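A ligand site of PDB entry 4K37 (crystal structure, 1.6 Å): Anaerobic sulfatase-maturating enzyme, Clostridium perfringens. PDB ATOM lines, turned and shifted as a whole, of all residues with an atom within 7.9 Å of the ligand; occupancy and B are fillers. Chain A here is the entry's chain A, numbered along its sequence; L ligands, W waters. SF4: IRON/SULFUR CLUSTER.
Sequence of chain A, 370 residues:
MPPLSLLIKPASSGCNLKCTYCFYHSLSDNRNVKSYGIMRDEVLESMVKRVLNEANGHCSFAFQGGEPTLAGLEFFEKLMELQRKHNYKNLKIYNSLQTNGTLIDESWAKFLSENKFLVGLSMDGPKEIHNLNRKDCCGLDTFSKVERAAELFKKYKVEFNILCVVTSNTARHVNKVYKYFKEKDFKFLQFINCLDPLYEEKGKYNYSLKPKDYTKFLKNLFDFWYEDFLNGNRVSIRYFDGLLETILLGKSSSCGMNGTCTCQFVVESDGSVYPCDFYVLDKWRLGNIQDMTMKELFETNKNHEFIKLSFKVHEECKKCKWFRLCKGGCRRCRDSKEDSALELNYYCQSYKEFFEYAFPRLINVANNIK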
ATOM      1  N   SER A 254     -14.282 -35.241   0.092  1.00  0.00           N
ATOM      2  CA  SER A 254     -14.545 -34.038  -0.702  1.00  0.00           C
ATOM      3  C   SER A 254     -13.424 -33.739  -1.689  1.00  0.00           C
ATOM      4  O   SER A 254     -12.253 -33.632  -1.323  1.00  0.00           O
ATOM      5  CB  SER A 254     -14.785 -32.818   0.181  1.00  0.00           C
ATOM      6  OG  SER A 254     -16.012 -32.938   0.890  1.00  0.00           O
ATOM      7  N   CYS A 255     -13.803 -33.603  -2.942  1.00  0.00           N
ATOM      8  CA  CYS A 255     -12.857 -33.238  -3.969  1.00  0.00           C
ATOM      9  C   CYS A 255     -12.291 -31.863  -3.659  1.00  0.00           C
ATOM     10  O   CYS A 255     -13.042 -30.917  -3.408  1.00  0.00           O
ATOM     11  CB  CYS A 255     -13.564 -33.227  -5.326  1.00  0.00           C
ATOM     12  SG  CYS A 255     -12.432 -33.340  -6.668  1.00  0.00           S
ATOM     13  N   GLY A 256     -10.963 -31.746  -3.689  1.00  0.00           N
ATOM     14  CA  GLY A 256     -10.305 -30.483  -3.422  1.00  0.00           C
ATOM     15  C   GLY A 256      -9.655 -30.481  -2.060  1.00  0.00           C
ATOM     16  O   GLY A 256      -8.966 -29.523  -1.679  1.00  0.00           O
ATOM     17  N   MET A 257      -9.903 -31.518  -1.261  1.00  0.00           N
ATOM     18  CA  MET A 257      -9.162 -31.568  -0.026  1.00  0.00           C
ATOM     19  C   MET A 257      -8.134 -32.723  -0.001  1.00  0.00           C
ATOM     20  O   MET A 257      -7.430 -32.882   0.971  1.00  0.00           O
ATOM     21  CB  MET A 257     -10.124 -31.563   1.173  1.00  0.00           C
ATOM     22  CG  MET A 257     -10.795 -30.213   1.592  1.00  0.00           C
ATOM     23  SD  MET A 257     -12.126 -30.468   2.777  1.00  0.00           S
ATOM     24  CE  MET A 257     -11.173 -30.457   4.297  1.00  0.00           C
ATOM     25  N   ASN A 258      -8.018 -33.506  -1.061  1.00  0.00           N
ATOM     26  CA  ASN A 258      -7.055 -34.596  -1.098  1.00  0.00           C
ATOM     27  C   ASN A 258      -5.778 -34.306  -1.873  1.00  0.00           C
ATOM     28  O   ASN A 258      -4.906 -35.175  -2.027  1.00  0.00           O
ATOM     29  CB  ASN A 258      -7.732 -35.865  -1.618  1.00  0.00           C
ATOM     30  CG  ASN A 258      -8.810 -36.367  -0.671  1.00  0.00           C
ATOM     31  OD1 ASN A 258      -8.610 -36.416   0.542  1.00  0.00           O
ATOM     32  ND2 ASN A 258      -9.965 -36.718  -1.229  1.00  0.00           N
ATOM     33  N   GLY A 259      -5.670 -33.084  -2.373  1.00  0.00           N
ATOM     34  CA  GLY A 259      -4.442 -32.629  -2.995  1.00  0.00           C
ATOM     35  C   GLY A 259      -4.346 -32.849  -4.489  1.00  0.00           C
ATOM     36  O   GLY A 259      -3.531 -32.218  -5.146  1.00  0.00           O
ATOM     37  N   THR A 260      -5.167 -33.756  -5.017  1.00  0.00           N
ATOM     38  CA  THR A 260      -5.205 -33.983  -6.469  1.00  0.00           C
ATOM     39  C   THR A 260      -6.628 -34.069  -6.999  1.00  0.00           C
ATOM     40  O   THR A 260      -7.569 -34.300  -6.242  1.00  0.00           O
ATOM     41  CB  THR A 260      -4.445 -35.254  -6.894  1.00  0.00           C
ATOM     42  OG1 THR A 260      -5.084 -36.408  -6.344  1.00  0.00           O
ATOM     43  CG2 THR A 260      -2.998 -35.207  -6.428  1.00  0.00           C
ATOM     44  N   CYS A 261      -6.779 -33.901  -8.308  1.00  0.00           N
ATOM     45  CA  CYS A 261      -8.091 -33.831  -8.938  1.00  0.00           C
ATOM     46  C   CYS A 261      -8.661 -35.195  -9.258  1.00  0.00           C
ATOM     47  O   CYS A 261      -7.944 -36.197  -9.268  1.00  0.00           O
ATOM     48  CB  CYS A 261      -8.014 -33.019 -10.235  1.00  0.00           C
ATOM     49  SG  CYS A 261      -7.576 -31.289  -9.958  1.00  0.00           S
ATOM     50  N   THR A 262      -9.966 -35.221  -9.518  1.00  0.00           N
ATOM     51  CA  THR A 262     -10.662 -36.413  -9.934  1.00  0.00           C
ATOM     52  C   THR A 262     -11.460 -36.064 -11.196  1.00  0.00           C
ATOM     53  O   THR A 262     -11.699 -34.897 -11.476  1.00  0.00           O
ATOM     54  CB  THR A 262     -11.684 -36.861  -8.859  1.00  0.00           C
ATOM     55  OG1 THR A 262     -12.641 -35.819  -8.652  1.00  0.00           O
ATOM     56  CG2 THR A 262     -10.982 -37.196  -7.549  1.00  0.00           C
ATOM     57  N   CYS A 263     -11.857 -37.068 -11.969  1.00  0.00           N
ATOM     58  CA  CYS A 263     -12.776 -36.817 -13.068  1.00  0.00           C
ATOM     59  C   CYS A 263     -14.224 -36.867 -12.581  1.00  0.00           C
ATOM     60  O   CYS A 263     -14.717 -37.919 -12.163  1.00  0.00           O
ATOM     61  CB  CYS A 263     -12.558 -37.830 -14.198  1.00  0.00           C
ATOM     62  SG  CYS A 263     -13.696 -37.588 -15.610  1.00  0.00           S
ATOM     63  N   GLN A 264     -14.917 -35.722 -12.638  1.00  0.00           N
ATOM     64  CA  GLN A 264     -16.279 -35.621 -12.128  1.00  0.00           C
ATOM     65  C   GLN A 264     -17.377 -35.962 -13.120  1.00  0.00           C
ATOM     66  O   GLN A 264     -18.541 -36.051 -12.748  1.00  0.00           O
ATOM     67  CB  GLN A 264     -16.533 -34.213 -11.572  1.00  0.00           C
ATOM     68  CG  GLN A 264     -15.443 -33.765 -10.592  1.00  0.00           C
ATOM     69  CD  GLN A 264     -15.718 -32.401 -10.013  1.00  0.00           C
ATOM     70  OE1 GLN A 264     -16.486 -31.610 -10.585  1.00  0.00           O
ATOM     71  NE2 GLN A 264     -15.097 -32.111  -8.867  1.00  0.00           N
ATOM     72  N   PRO A 275     -14.051 -32.736 -17.146  1.00  0.00           N
ATOM     73  CA  PRO A 275     -13.565 -33.409 -15.932  1.00  0.00           C
ATOM     74  C   PRO A 275     -13.982 -32.749 -14.614  1.00  0.00           C
ATOM     75  O   PRO A 275     -13.970 -33.409 -13.566  1.00  0.00           O
ATOM     76  CB  PRO A 275     -12.034 -33.368 -16.110  1.00  0.00           C
ATOM     77  CG  PRO A 275     -11.793 -32.157 -16.946  1.00  0.00           C
ATOM     78  CD  PRO A 275     -12.987 -32.035 -17.870  1.00  0.00           C
ATOM     79  N   CYS A 276     -14.354 -31.469 -14.652  1.00  0.00           N
ATOM     80  CA  CYS A 276     -14.644 -30.741 -13.432  1.00  0.00           C
ATOM     81  C   CYS A 276     -15.557 -29.566 -13.732  1.00  0.00           C
ATOM     82  O   CYS A 276     -15.462 -28.939 -14.782  1.00  0.00           O
ATOM     83  CB  CYS A 276     -13.348 -30.228 -12.779  1.00  0.00           C
ATOM     84  SG  CYS A 276     -13.611 -29.171 -11.326  1.00  0.00           S
ATOM     85  N   ASP A 277     -16.474 -29.250 -12.837  1.00  0.00           N
ATOM     86  CA  ASP A 277     -17.479 -28.195 -13.122  1.00  0.00           C
ATOM     87  C   ASP A 277     -16.827 -26.769 -13.159  1.00  0.00           C
ATOM     88  O   ASP A 277     -17.389 -25.848 -13.684  1.00  0.00           O
ATOM     89  CB  ASP A 277     -18.728 -28.412 -12.213  1.00  0.00           C
ATOM     90  CG  ASP A 277     -19.492 -27.214 -11.914  1.00  0.00           C
ATOM     91  OD1 ASP A 277     -20.078 -26.635 -12.854  1.00  0.00           O
ATOM     92  OD2 ASP A 277     -19.531 -26.862 -10.705  1.00  0.00           O
ATOM     93  N   PHE A 278     -15.584 -26.674 -12.694  1.00  0.00           N
ATOM     94  CA  PHE A 278     -14.841 -25.406 -12.868  1.00  0.00           C
ATOM     95  C   PHE A 278     -14.206 -25.321 -14.246  1.00  0.00           C
ATOM     96  O   PHE A 278     -13.665 -24.269 -14.612  1.00  0.00           O
ATOM     97  CB  PHE A 278     -13.712 -25.286 -11.840  1.00  0.00           C
ATOM     98  CG  PHE A 278     -14.163 -25.168 -10.421  1.00  0.00           C
ATOM     99  CD1 PHE A 278     -15.177 -24.276 -10.068  1.00  0.00           C
ATOM    100  CD2 PHE A 278     -13.584 -25.945  -9.431  1.00  0.00           C
ATOM    101  CE1 PHE A 278     -15.591 -24.164  -8.755  1.00  0.00           C
ATOM    102  CE2 PHE A 278     -13.997 -25.837  -8.105  1.00  0.00           C
ATOM    103  CZ  PHE A 278     -15.006 -24.936  -7.771  1.00  0.00           C
ATOM    104  N   TYR A 279     -14.229 -26.426 -14.990  1.00  0.00           N
ATOM    105  CA  TYR A 279     -13.464 -26.520 -16.238  1.00  0.00           C
ATOM    106  C   TYR A 279     -14.307 -26.988 -17.424  1.00  0.00           C
ATOM    107  O   TYR A 279     -13.869 -27.807 -18.258  1.00  0.00           O
ATOM    108  CB  TYR A 279     -12.248 -27.430 -16.028  1.00  0.00           C
ATOM    109  CG  TYR A 279     -11.183 -26.790 -15.174  1.00  0.00           C
ATOM    110  CD1 TYR A 279     -10.242 -25.927 -15.723  1.00  0.00           C
ATOM    111  CD2 TYR A 279     -11.136 -27.027 -13.797  1.00  0.00           C
ATOM    112  CE1 TYR A 279      -9.276 -25.324 -14.940  1.00  0.00           C
ATOM    113  CE2 TYR A 279     -10.164 -26.422 -13.006  1.00  0.00           C
ATOM    114  CZ  TYR A 279      -9.242 -25.572 -13.589  1.00  0.00           C
ATOM    115  OH  TYR A 279      -8.276 -24.969 -12.805  1.00  0.00           O
ATOM    116  N   PHE A 306      -5.554 -33.464 -17.489  1.00  0.00           N
ATOM    117  CA  PHE A 306      -6.219 -32.711 -16.439  1.00  0.00           C
ATOM    118  C   PHE A 306      -5.803 -33.204 -15.045  1.00  0.00           C
ATOM    119  O   PHE A 306      -5.372 -32.410 -14.188  1.00  0.00           O
ATOM    120  CB  PHE A 306      -7.750 -32.762 -16.581  1.00  0.00           C
ATOM    121  CG  PHE A 306      -8.454 -31.927 -15.565  1.00  0.00           C
ATOM    122  CD1 PHE A 306      -8.594 -30.550 -15.751  1.00  0.00           C
ATOM    123  CD2 PHE A 306      -8.963 -32.497 -14.401  1.00  0.00           C
ATOM    124  CE1 PHE A 306      -9.231 -29.773 -14.805  1.00  0.00           C
ATOM    125  CE2 PHE A 306      -9.594 -31.719 -13.447  1.00  0.00           C
ATOM    126  CZ  PHE A 306      -9.735 -30.352 -13.643  1.00  0.00           C
ATOM    127  N   ILE A 307      -5.893 -34.509 -14.829  1.00  0.00           N
ATOM    128  CA  ILE A 307      -5.596 -35.070 -13.522  1.00  0.00           C
ATOM    129  C   ILE A 307      -4.106 -35.020 -13.180  1.00  0.00           C
ATOM    130  O   ILE A 307      -3.750 -34.701 -12.048  1.00  0.00           O
ATOM    131  CB  ILE A 307      -6.104 -36.514 -13.416  1.00  0.00           C
ATOM    132  CG1 ILE A 307      -7.634 -36.527 -13.487  1.00  0.00           C
ATOM    133  CG2 ILE A 307      -5.623 -37.141 -12.128  1.00  0.00           C
ATOM    134  CD1 ILE A 307      -8.232 -37.877 -13.234  1.00  0.00           C
ATOM    135  N   SER A 310      -2.428 -31.927 -11.725  1.00  0.00           N
ATOM    136  CA  SER A 310      -2.735 -31.645 -10.331  1.00  0.00           C
ATOM    137  C   SER A 310      -1.805 -32.287  -9.306  1.00  0.00           C
ATOM    138  O   SER A 310      -1.893 -32.009  -8.149  1.00  0.00           O
ATOM    139  CB  SER A 310      -4.184 -32.012  -9.985  1.00  0.00           C
ATOM    140  OG  SER A 310      -4.334 -33.366  -9.689  1.00  0.00           O
ATOM    141  N   GLY A 329      -4.577 -27.852  -1.233  1.00  0.00           N
ATOM    142  CA  GLY A 329      -5.908 -27.372  -1.553  1.00  0.00           C
ATOM    143  C   GLY A 329      -6.389 -27.756  -2.950  1.00  0.00           C
ATOM    144  O   GLY A 329      -5.803 -28.596  -3.627  1.00  0.00           O
ATOM    145  N   CYS A 330      -7.457 -27.100  -3.378  1.00  0.00           N
ATOM    146  CA  CYS A 330      -8.099 -27.384  -4.663  1.00  0.00           C
ATOM    147  C   CYS A 330      -7.290 -26.788  -5.811  1.00  0.00           C
ATOM    148  O   CYS A 330      -6.871 -25.634  -5.762  1.00  0.00           O
ATOM    149  CB  CYS A 330      -9.508 -26.795  -4.669  1.00  0.00           C
ATOM    150  SG  CYS A 330     -10.372 -26.771  -6.251  1.00  0.00           S
ATOM    151  N   ARG A 331      -7.099 -27.577  -6.865  1.00  0.00           N
ATOM    152  CA  ARG A 331      -6.334 -27.124  -8.020  1.00  0.00           C
ATOM    153  C   ARG A 331      -6.897 -25.834  -8.655  1.00  0.00           C
ATOM    154  O   ARG A 331      -6.148 -25.034  -9.209  1.00  0.00           O
ATOM    155  CB  ARG A 331      -6.265 -28.267  -9.050  1.00  0.00           C
ATOM    156  CG  ARG A 331      -5.803 -27.830 -10.424  1.00  0.00           C
ATOM    157  CD  ARG A 331      -6.955 -27.772 -11.450  1.00  0.00           C
ATOM    158  NE  ARG A 331      -6.397 -27.826 -12.796  1.00  0.00           N
ATOM    159  CZ  ARG A 331      -6.083 -28.963 -13.417  1.00  0.00           C
ATOM    160  NH1 ARG A 331      -6.319 -30.108 -12.828  1.00  0.00           N
ATOM    161  NH2 ARG A 331      -5.554 -28.940 -14.637  1.00  0.00           N
ATOM    162  N   ARG A 332      -8.203 -25.632  -8.564  1.00  0.00           N
ATOM    163  CA  ARG A 332      -8.795 -24.460  -9.183  1.00  0.00           C
ATOM    164  C   ARG A 332      -8.246 -23.176  -8.524  1.00  0.00           C
ATOM    165  O   ARG A 332      -8.153 -22.128  -9.151  1.00  0.00           O
ATOM    166  CB  ARG A 332     -10.321 -24.540  -9.104  1.00  0.00           C
ATOM    167  CG  ARG A 332     -11.058 -23.258  -9.497  1.00  0.00           C
ATOM    168  CD  ARG A 332     -10.817 -22.854 -10.948  1.00  0.00           C
ATOM    169  NE  ARG A 332     -11.653 -21.700 -11.306  1.00  0.00           N
ATOM    170  CZ  ARG A 332     -11.394 -20.442 -10.966  1.00  0.00           C
ATOM    171  NH1 ARG A 332     -12.214 -19.477 -11.345  1.00  0.00           N
ATOM    172  NH2 ARG A 332     -10.305 -20.156 -10.242  1.00  0.00           N
ATOM    173  N   CYS A 333      -7.808 -23.303  -7.269  1.00  0.00           N
ATOM    174  CA  CYS A 333      -7.255 -22.162  -6.565  1.00  0.00           C
ATOM    175  C   CYS A 333      -5.752 -21.991  -6.793  1.00  0.00           C
ATOM    176  O   CYS A 333      -5.133 -21.075  -6.247  1.00  0.00           O
ATOM    177  CB  CYS A 333      -7.569 -22.273  -5.076  1.00  0.00           C
ATOM    178  SG  CYS A 333      -9.303 -21.907  -4.699  1.00  0.00           S
ATOM    179  N   ARG A 334      -5.186 -22.870  -7.616  1.00  0.00           N
ATOM    180  CA  ARG A 334      -3.756 -22.876  -7.913  1.00  0.00           C
ATOM    181  C   ARG A 334      -3.523 -22.488  -9.369  1.00  0.00           C
ATOM    182  O   ARG A 334      -2.390 -22.288  -9.810  1.00  0.00           O
ATOM    183  CB  ARG A 334      -3.168 -24.264  -7.656  1.00  0.00           C
ATOM    184  CG  ARG A 334      -3.267 -24.759  -6.225  1.00  0.00           C
ATOM    185  CD  ARG A 334      -2.574 -26.118  -6.056  1.00  0.00           C
ATOM    186  NE  ARG A 334      -1.176 -26.060  -6.466  1.00  0.00           N
ATOM    187  CZ  ARG A 334      -0.407 -27.124  -6.687  1.00  0.00           C
ATOM    188  NH1 ARG A 334      -0.890 -28.350  -6.507  1.00  0.00           N
ATOM    189  NH2 ARG A 334       0.846 -26.958  -7.064  1.00  0.00           N
ATOM    190  N   ASP A 335      -4.616 -22.394 -10.125  1.00  0.00           N
ATOM    191  CA  ASP A 335      -4.553 -22.251 -11.574  1.00  0.00           C
ATOM    192  C   ASP A 335      -4.698 -20.791 -12.001  1.00  0.00           C
ATOM    193  O   ASP A 335      -5.790 -20.312 -12.292  1.00  0.00           O
ATOM    194  CB  ASP A 335      -5.641 -23.128 -12.205  1.00  0.00           C
ATOM    195  CG  ASP A 335      -5.417 -23.349 -13.684  1.00  0.00           C
ATOM    196  OD1 ASP A 335      -4.347 -22.994 -14.204  1.00  0.00           O
ATOM    197  OD2 ASP A 335      -6.334 -23.904 -14.335  1.00  0.00           O
HETATM  198 FE1  SF4 L   1     -12.085 -29.695  -9.622  1.00  0.00          FE
HETATM  199 FE2  SF4 L   1     -11.618 -31.347  -7.516  1.00  0.00          FE
HETATM  200 FE3  SF4 L   1      -9.568 -30.514  -9.094  1.00  0.00          FE
HETATM  201 FE4  SF4 L   1     -10.780 -28.762  -7.384  1.00  0.00          FE
HETATM  202  S1  SF4 L   1      -9.589 -30.599  -6.813  1.00  0.00           S
HETATM  203  S2  SF4 L   1     -10.233 -28.375  -9.565  1.00  0.00           S
HETATM  204  S3  SF4 L   1     -12.935 -29.485  -7.503  1.00  0.00           S
HETATM  205  S4  SF4 L   1     -11.321 -31.827  -9.732  1.00  0.00           S
HETATM  206  O   HOH W   1      -6.359 -30.754  -6.778  1.00  0.00           O
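The side-chain sulfur of Cys 261 is bound to an iron atom (FE3) of the ligand (2.3 Å).
The side-chain sulfur of Cys 255 is bound to an iron atom (FE2) of the ligand (2.3 Å).
The side-chain sulfur (SG) of Cys 330 binds an iron atom (FE4) of the ligand.
FE1 of the ligand is bound by SG of Cys 276 (2.3 Å).
The backbone NH of Gly 256 lies close to a sulfur (S1) of the ligand, 3.6 Å away.
The backbone NH (N) of Thr 262 sits close to a sulfur (S4) of the ligand (3.7 Å).
The backbone NH of Arg 332 sits close to a sulfur (S2) of the ligand, at 3.6 Å.
The side-chain amide nitrogen of Gln 264 lies close to a sulfur (S3) of the ligand, at 3.7 Å.
SG of Cys 261 sits close to NH1 of Arg 331, 3.3 Å away.
The side-chain sulfur of Cys 255 sits close to the side-chain hydroxyl of Thr 262.
The backbone NH (N) of Cys 330 lies within hydrogen-bond range of the backbone carbonyl oxygen (O) of Gly 256 (3.3 Å).
The side-chain sulfur (SG) of Cys 330 lies close to the backbone NH (N) of Arg 332 (3.4 Å).
The backbone NH of Phe 278 lies close to the side-chain sulfur of Cys 276.
The side-chain amide oxygen (OE1) of Gln 264 lies within hydrogen-bond range of the backbone NH (N) of Asp 277, at 3.3 Å.
NH1 of Arg 331 lies within hydrogen-bond range of O of Phe 306 (2.8 Å).
The side-chain carboxylate (OD2) of Asp 335 lies within hydrogen-bond range of the side-chain hydroxyl (OH) of Tyr 279, at 2.7 Å.
CE2 of Phe 278 touches S3 of the ligand, at 3.8 Å.
Tyr 279 touches the ligand (CE2 to S2, 3.96 Å).
CD of Arg 331 touches S2 of the ligand, at 3.8 Å.
Of the 26 residues printed, 11 come within 4 Å of the ligand.
Along chain A the residues within 4 Å of the ligand span positions 255 to 332.
Water W1 bridges a sulfur (S1) of the ligand (3.2 Å) and the backbone NH (N) of Arg 331 (3.3 Å).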
